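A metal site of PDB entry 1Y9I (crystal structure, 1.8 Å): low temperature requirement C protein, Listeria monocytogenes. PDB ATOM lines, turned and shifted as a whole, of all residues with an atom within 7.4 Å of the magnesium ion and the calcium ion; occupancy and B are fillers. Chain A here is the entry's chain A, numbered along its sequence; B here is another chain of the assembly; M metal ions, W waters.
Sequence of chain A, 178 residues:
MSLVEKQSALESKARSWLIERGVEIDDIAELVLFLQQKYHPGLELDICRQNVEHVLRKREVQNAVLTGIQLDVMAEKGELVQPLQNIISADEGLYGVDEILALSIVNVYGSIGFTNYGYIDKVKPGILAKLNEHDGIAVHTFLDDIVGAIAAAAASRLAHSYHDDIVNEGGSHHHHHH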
ATOM      1  N   ASP A  72       6.306 -17.524  22.784  1.00  0.00           N
ATOM      2  CA  ASP A  72       6.985 -16.701  21.773  1.00  0.00           C
ATOM      3  C   ASP A  72       6.567 -17.127  20.369  1.00  0.00           C
ATOM      4  O   ASP A  72       6.238 -16.285  19.511  1.00  0.00           O
ATOM      5  CB  ASP A  72       8.504 -16.874  21.845  1.00  0.00           C
ATOM      6  CG  ASP A  72       9.112 -16.183  23.043  1.00  0.00           C
ATOM      7  OD1 ASP A  72       8.431 -15.334  23.653  1.00  0.00           O
ATOM      8  OD2 ASP A  72      10.285 -16.491  23.359  1.00  0.00           O
ATOM      9  N   ASP A  91       6.818  -7.059  22.945  1.00  0.00           N
ATOM     10  CA  ASP A  91       7.668  -7.065  24.139  1.00  0.00           C
ATOM     11  C   ASP A  91       7.381  -5.846  25.017  1.00  0.00           C
ATOM     12  O   ASP A  91       8.301  -5.137  25.436  1.00  0.00           O
ATOM     13  CB  ASP A  91       9.140  -7.101  23.720  1.00  0.00           C
ATOM     14  CG  ASP A  91      10.076  -7.407  24.884  1.00  0.00           C
ATOM     15  OD1 ASP A  91       9.592  -7.711  25.995  1.00  0.00           O
ATOM     16  OD2 ASP A  91      11.308  -7.344  24.668  1.00  0.00           O
ATOM     17  N   GLU A  92       6.098  -5.603  25.288  1.00  0.00           N
ATOM     18  CA  GLU A  92       5.645  -4.483  26.112  1.00  0.00           C
ATOM     19  C   GLU A  92       6.430  -4.366  27.403  1.00  0.00           C
ATOM     20  O   GLU A  92       6.591  -5.342  28.137  1.00  0.00           O
ATOM     21  CB  GLU A  92       4.167  -4.663  26.446  1.00  0.00           C
ATOM     22  CG  GLU A  92       3.280  -3.514  26.004  1.00  0.00           C
ATOM     23  CD  GLU A  92       1.821  -3.734  26.378  1.00  0.00           C
ATOM     24  OE1 GLU A  92       1.529  -3.878  27.593  1.00  0.00           O
ATOM     25  OE2 GLU A  92       0.969  -3.747  25.461  1.00  0.00           O
ATOM     26  N   GLY A  93       6.921  -3.154  27.685  1.00  0.00           N
ATOM     27  CA  GLY A  93       7.696  -2.929  28.885  1.00  0.00           C
ATOM     28  C   GLY A  93       6.999  -3.223  30.202  1.00  0.00           C
ATOM     29  O   GLY A  93       7.651  -3.610  31.172  1.00  0.00           O
ATOM     30  N   LEU A  94       5.682  -3.054  30.243  1.00  0.00           N
ATOM     31  CA  LEU A  94       4.964  -3.307  31.496  1.00  0.00           C
ATOM     32  C   LEU A  94       4.451  -4.738  31.641  1.00  0.00           C
ATOM     33  O   LEU A  94       3.749  -5.055  32.615  1.00  0.00           O
ATOM     34  CB  LEU A  94       3.823  -2.299  31.655  1.00  0.00           C
ATOM     35  CG  LEU A  94       4.306  -0.833  31.691  1.00  0.00           C
ATOM     36  CD1 LEU A  94       3.124   0.087  31.976  1.00  0.00           C
ATOM     37  CD2 LEU A  94       5.374  -0.656  32.768  1.00  0.00           C
ATOM     38  N   TYR A  95       4.781  -5.605  30.693  1.00  0.00           N
ATOM     39  CA  TYR A  95       4.390  -7.007  30.757  1.00  0.00           C
ATOM     40  C   TYR A  95       5.564  -7.716  31.440  1.00  0.00           C
ATOM     41  O   TYR A  95       6.669  -7.776  30.895  1.00  0.00           O
ATOM     42  CB  TYR A  95       4.177  -7.570  29.354  1.00  0.00           C
ATOM     43  CG  TYR A  95       3.775  -9.029  29.320  1.00  0.00           C
ATOM     44  CD1 TYR A  95       2.468  -9.430  29.627  1.00  0.00           C
ATOM     45  CD2 TYR A  95       4.700 -10.005  28.943  1.00  0.00           C
ATOM     46  CE1 TYR A  95       2.094 -10.784  29.561  1.00  0.00           C
ATOM     47  CE2 TYR A  95       4.332 -11.358  28.861  1.00  0.00           C
ATOM     48  CZ  TYR A  95       3.033 -11.736  29.171  1.00  0.00           C
ATOM     49  OH  TYR A  95       2.691 -13.076  29.068  1.00  0.00           O
ATOM     50  N   GLY A  96       5.321  -8.253  32.623  1.00  0.00           N
ATOM     51  CA  GLY A  96       6.412  -8.912  33.336  1.00  0.00           C
ATOM     52  C   GLY A  96       6.272 -10.396  33.560  1.00  0.00           C
ATOM     53  O   GLY A  96       6.962 -10.954  34.409  1.00  0.00           O
ATOM     54  N   VAL A  97       5.407 -11.061  32.798  1.00  0.00           N
ATOM     55  CA  VAL A  97       5.222 -12.494  32.975  1.00  0.00           C
ATOM     56  C   VAL A  97       6.464 -13.243  32.503  1.00  0.00           C
ATOM     57  O   VAL A  97       6.808 -14.285  33.059  1.00  0.00           O
ATOM     58  CB  VAL A  97       3.951 -13.006  32.246  1.00  0.00           C
ATOM     59  CG1 VAL A  97       3.791 -14.508  32.462  1.00  0.00           C
ATOM     60  CG2 VAL A  97       2.716 -12.287  32.791  1.00  0.00           C
ATOM     61  N   ASP A  98       7.168 -12.703  31.503  1.00  0.00           N
ATOM     62  CA  ASP A  98       8.375 -13.356  31.009  1.00  0.00           C
ATOM     63  C   ASP A  98       9.484 -13.322  32.071  1.00  0.00           C
ATOM     64  O   ASP A  98      10.233 -14.288  32.209  1.00  0.00           O
ATOM     65  CB  ASP A  98       8.873 -12.723  29.677  1.00  0.00           C
ATOM     66  CG  ASP A  98       8.883 -11.200  29.682  1.00  0.00           C
ATOM     67  OD1 ASP A  98       7.879 -10.582  30.081  1.00  0.00           O
ATOM     68  OD2 ASP A  98       9.915 -10.615  29.271  1.00  0.00           O
ATOM     69  N   GLU A  99       9.553 -12.242  32.840  1.00  0.00           N
ATOM     70  CA  GLU A  99      10.554 -12.126  33.897  1.00  0.00           C
ATOM     71  C   GLU A  99      10.196 -13.055  35.070  1.00  0.00           C
ATOM     72  O   GLU A  99      11.077 -13.585  35.762  1.00  0.00           O
ATOM     73  CB  GLU A  99      10.649 -10.692  34.409  1.00  0.00           C
ATOM     74  CG  GLU A  99      11.348  -9.701  33.452  1.00  0.00           C
ATOM     75  CD  GLU A  99      10.436  -9.148  32.357  1.00  0.00           C
ATOM     76  OE1 GLU A  99       9.257  -9.527  32.281  1.00  0.00           O
ATOM     77  OE2 GLU A  99      10.913  -8.313  31.568  1.00  0.00           O
ATOM     78  N   ILE A 100       8.906 -13.258  35.293  1.00  0.00           N
ATOM     79  CA  ILE A 100       8.432 -14.134  36.372  1.00  0.00           C
ATOM     80  C   ILE A 100       8.795 -15.580  36.085  1.00  0.00           C
ATOM     81  O   ILE A 100       9.329 -16.287  36.939  1.00  0.00           O
ATOM     82  CB  ILE A 100       6.886 -14.013  36.537  1.00  0.00           C
ATOM     83  CG1 ILE A 100       6.530 -12.694  37.218  1.00  0.00           C
ATOM     84  CG2 ILE A 100       6.333 -15.197  37.295  1.00  0.00           C
ATOM     85  CD1 ILE A 100       6.988 -12.599  38.653  1.00  0.00           C
ATOM     86  N   TYR A 117      20.993 -12.149  37.097  1.00  0.00           N
ATOM     87  CA  TYR A 117      19.866 -12.260  36.182  1.00  0.00           C
ATOM     88  C   TYR A 117      19.473 -10.854  35.697  1.00  0.00           C
ATOM     89  O   TYR A 117      19.351 -10.616  34.490  1.00  0.00           O
ATOM     90  CB  TYR A 117      18.708 -12.930  36.905  1.00  0.00           C
ATOM     91  CG  TYR A 117      17.374 -12.936  36.193  1.00  0.00           C
ATOM     92  CD1 TYR A 117      17.248 -13.443  34.895  1.00  0.00           C
ATOM     93  CD2 TYR A 117      16.206 -12.523  36.846  1.00  0.00           C
ATOM     94  CE1 TYR A 117      16.008 -13.542  34.273  1.00  0.00           C
ATOM     95  CE2 TYR A 117      14.965 -12.616  36.237  1.00  0.00           C
ATOM     96  CZ  TYR A 117      14.863 -13.126  34.958  1.00  0.00           C
ATOM     97  OH  TYR A 117      13.624 -13.255  34.376  1.00  0.00           O
ATOM     98  N   ASP A 121      20.424  -9.037  31.886  1.00  0.00           N
ATOM     99  CA  ASP A 121      19.277  -8.643  31.081  1.00  0.00           C
ATOM    100  C   ASP A 121      19.436  -7.208  30.586  1.00  0.00           C
ATOM    101  O   ASP A 121      18.939  -6.850  29.506  1.00  0.00           O
ATOM    102  CB  ASP A 121      17.992  -8.756  31.902  1.00  0.00           C
ATOM    103  CG  ASP A 121      16.763  -8.398  31.085  1.00  0.00           C
ATOM    104  OD1 ASP A 121      16.473  -9.132  30.119  1.00  0.00           O
ATOM    105  OD2 ASP A 121      16.099  -7.383  31.403  1.00  0.00           O
ATOM    106  N   LYS A 124      22.834  -7.286  28.094  1.00  0.00           N
ATOM    107  CA  LYS A 124      22.582  -8.097  26.921  1.00  0.00           C
ATOM    108  C   LYS A 124      23.816  -8.409  26.071  1.00  0.00           C
ATOM    109  O   LYS A 124      23.862  -8.092  24.882  1.00  0.00           O
ATOM    110  CB  LYS A 124      21.526  -7.428  26.043  1.00  0.00           C
ATOM    111  CG  LYS A 124      20.229  -7.139  26.780  1.00  0.00           C
ATOM    112  CD  LYS A 124      19.202  -6.466  25.893  1.00  0.00           C
ATOM    113  CE  LYS A 124      17.924  -6.181  26.666  1.00  0.00           C
ATOM    114  NZ  LYS A 124      17.330  -7.426  27.212  1.00  0.00           N
ATOM    115  N   HIS A 140      11.062 -12.954  20.839  1.00  0.00           N
ATOM    116  CA  HIS A 140      11.885 -13.622  21.837  1.00  0.00           C
ATOM    117  C   HIS A 140      11.614 -13.040  23.221  1.00  0.00           C
ATOM    118  O   HIS A 140      12.488 -12.993  24.081  1.00  0.00           O
ATOM    119  CB  HIS A 140      13.371 -13.448  21.498  1.00  0.00           C
ATOM    120  CG  HIS A 140      13.780 -14.137  20.224  1.00  0.00           C
ATOM    121  ND1 HIS A 140      13.812 -15.507  20.098  1.00  0.00           N
ATOM    122  CD2 HIS A 140      14.176 -13.639  19.032  1.00  0.00           C
ATOM    123  CE1 HIS A 140      14.212 -15.825  18.878  1.00  0.00           C
ATOM    124  NE2 HIS A 140      14.433 -14.713  18.210  1.00  0.00           N
ATOM    125  N   THR A 141      10.375 -12.588  23.411  1.00  0.00           N
ATOM    126  CA  THR A 141       9.940 -11.989  24.652  1.00  0.00           C
ATOM    127  C   THR A 141      10.226 -12.881  25.857  1.00  0.00           C
ATOM    128  O   THR A 141      10.691 -12.405  26.897  1.00  0.00           O
ATOM    129  CB  THR A 141       8.434 -11.692  24.569  1.00  0.00           C
ATOM    130  OG1 THR A 141       8.205 -10.743  23.514  1.00  0.00           O
ATOM    131  CG2 THR A 141       7.917 -11.123  25.886  1.00  0.00           C
ATOM    132  N   PHE A 142       9.976 -14.176  25.719  1.00  0.00           N
ATOM    133  CA  PHE A 142      10.231 -15.107  26.815  1.00  0.00           C
ATOM    134  C   PHE A 142      11.629 -15.715  26.761  1.00  0.00           C
ATOM    135  O   PHE A 142      12.265 -15.934  27.799  1.00  0.00           O
ATOM    136  CB  PHE A 142       9.210 -16.228  26.802  1.00  0.00           C
ATOM    137  CG  PHE A 142       7.883 -15.826  27.336  1.00  0.00           C
ATOM    138  CD1 PHE A 142       7.587 -15.994  28.694  1.00  0.00           C
ATOM    139  CD2 PHE A 142       6.931 -15.241  26.504  1.00  0.00           C
ATOM    140  CE1 PHE A 142       6.371 -15.565  29.206  1.00  0.00           C
ATOM    141  CE2 PHE A 142       5.713 -14.798  27.016  1.00  0.00           C
ATOM    142  CZ  PHE A 142       5.434 -14.963  28.373  1.00  0.00           C
ATOM    143  N   LEU A 143      12.119 -15.975  25.556  1.00  0.00           N
ATOM    144  CA  LEU A 143      13.426 -16.581  25.407  1.00  0.00           C
ATOM    145  C   LEU A 143      14.595 -15.739  25.915  1.00  0.00           C
ATOM    146  O   LEU A 143      15.569 -16.293  26.441  1.00  0.00           O
ATOM    147  CB  LEU A 143      13.673 -16.964  23.945  1.00  0.00           C
ATOM    148  CG  LEU A 143      14.993 -17.696  23.688  1.00  0.00           C
ATOM    149  CD1 LEU A 143      15.084 -18.924  24.587  1.00  0.00           C
ATOM    150  CD2 LEU A 143      15.093 -18.111  22.225  1.00  0.00           C
ATOM    151  N   ASP A 144      14.535 -14.419  25.767  1.00  0.00           N
ATOM    152  CA  ASP A 144      15.639 -13.608  26.264  1.00  0.00           C
ATOM    153  C   ASP A 144      15.810 -13.779  27.776  1.00  0.00           C
ATOM    154  O   ASP A 144      16.941 -13.918  28.255  1.00  0.00           O
ATOM    155  CB  ASP A 144      15.510 -12.117  25.888  1.00  0.00           C
ATOM    156  CG  ASP A 144      14.157 -11.528  26.197  1.00  0.00           C
ATOM    157  OD1 ASP A 144      13.426 -12.063  27.055  1.00  0.00           O
ATOM    158  OD2 ASP A 144      13.814 -10.499  25.567  1.00  0.00           O
ATOM    159  N   ASP A 145      14.703 -13.781  28.516  1.00  0.00           N
ATOM    160  CA  ASP A 145      14.739 -13.959  29.967  1.00  0.00           C
ATOM    161  C   ASP A 145      15.216 -15.362  30.302  1.00  0.00           C
ATOM    162  O   ASP A 145      15.995 -15.570  31.247  1.00  0.00           O
ATOM    163  CB  ASP A 145      13.353 -13.783  30.582  1.00  0.00           C
ATOM    164  CG  ASP A 145      12.763 -12.423  30.310  1.00  0.00           C
ATOM    165  OD1 ASP A 145      13.209 -11.447  30.937  1.00  0.00           O
ATOM    166  OD2 ASP A 145      11.849 -12.340  29.465  1.00  0.00           O
ATOM    167  N   ILE A 146      14.733 -16.349  29.542  1.00  0.00           N
ATOM    168  CA  ILE A 146      15.111 -17.738  29.774  1.00  0.00           C
ATOM    169  C   ILE A 146      16.619 -17.938  29.658  1.00  0.00           C
ATOM    170  O   ILE A 146      17.246 -18.571  30.510  1.00  0.00           O
ATOM    171  CB  ILE A 146      14.378 -18.662  28.767  1.00  0.00           C
ATOM    172  CG1 ILE A 146      12.901 -18.777  29.156  1.00  0.00           C
ATOM    173  CG2 ILE A 146      15.049 -20.025  28.731  1.00  0.00           C
ATOM    174  CD1 ILE A 146      12.030 -19.517  28.119  1.00  0.00           C
ATOM    175  N   SER B 111       7.426  -7.592  38.842  1.00  0.00           N
ATOM    176  CA  SER B 111       8.609  -8.220  38.275  1.00  0.00           C
ATOM    177  C   SER B 111       9.385  -7.345  37.299  1.00  0.00           C
ATOM    178  O   SER B 111      10.568  -7.619  37.031  1.00  0.00           O
ATOM    179  CB  SER B 111       8.210  -9.516  37.561  1.00  0.00           C
ATOM    180  OG  SER B 111       7.196  -9.233  36.607  1.00  0.00           O
ATOM    181  N   ILE B 112       8.757  -6.315  36.754  1.00  0.00           N
ATOM    182  CA  ILE B 112       9.445  -5.435  35.817  1.00  0.00           C
ATOM    183  C   ILE B 112      10.558  -4.648  36.521  1.00  0.00           C
ATOM    184  O   ILE B 112      11.349  -3.949  35.877  1.00  0.00           O
ATOM    185  CB  ILE B 112       8.479  -4.439  35.137  1.00  0.00           C
ATOM    186  CG1 ILE B 112       7.794  -3.571  36.197  1.00  0.00           C
ATOM    187  CG2 ILE B 112       7.449  -5.209  34.308  1.00  0.00           C
ATOM    188  CD1 ILE B 112       6.858  -2.529  35.615  1.00  0.00           C
HETATM  189 MG    MG M   1      11.449 -10.860  27.969  1.00  0.00          MG
HETATM  190 CA    CA M   2       8.850  -8.344  30.123  1.00  0.00          CA
HETATM  191  O   HOH W   1      12.668  -9.757  29.235  1.00  0.00           O
HETATM  192  O   HOH W   2       9.120  -5.986  30.794  1.00  0.00           O
HETATM  193  O   HOH W   3      10.774  -7.638  28.656  1.00  0.00           O
HETATM  194  O   HOH W   4      11.685  -9.531  26.519  1.00  0.00           O
HETATM  195  O   HOH W   5       7.782  -7.906  28.021  1.00  0.00           O
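O of Glu 99 lies within hydrogen-bond range of OH of Tyr 117, at 2.9 Å.
The backbone NH (N) of Thr 141 is in hydrogen-bond range of the side-chain carboxylate (OD1) of Asp 72.
Within 4 Å of the magnesium ion: Asp 98, Thr 141, Asp 144 and Asp 145.
Along chain A the residues within 4 Å of the magnesium ion span positions 98 to 145.
The nearest printed residue that does not touch the magnesium ion is Asp 91 (4.2 Å).
The magnesium ion is bound by water W4 (2.0 Å).
O of Thr 141 binds the magnesium ion (2.0 Å).
OD2 of Asp 98 binds the magnesium ion (2.0 Å).
Water W1 is bound to the magnesium ion (2.1 Å).
The magnesium ion is bound by OD2 of Asp 145, at 2.1 Å.
The magnesium ion is bound by OD1 of Asp 144, at 2.5 Å.
The calcium ion is bound by O of Tyr 95 (2.4 Å), water W5 (2.4 Å), OD1 of Asp 98 (2.4 Å), water W2 (2.5 Å), OE1 of Glu 99 (2.5 Å), OE2 of Glu 99 (2.5 Å), water W3 (2.5 Å) and OD2 of Asp 98 (2.6 Å).
Water W4 lies within hydrogen-bond range of OD2 of Asp 144 (2.5 Å) and OD1 of Asp 91 (2.8 Å).
Water W5 lies within hydrogen-bond range of OD1 of Asp 91 and O of Glu 92.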
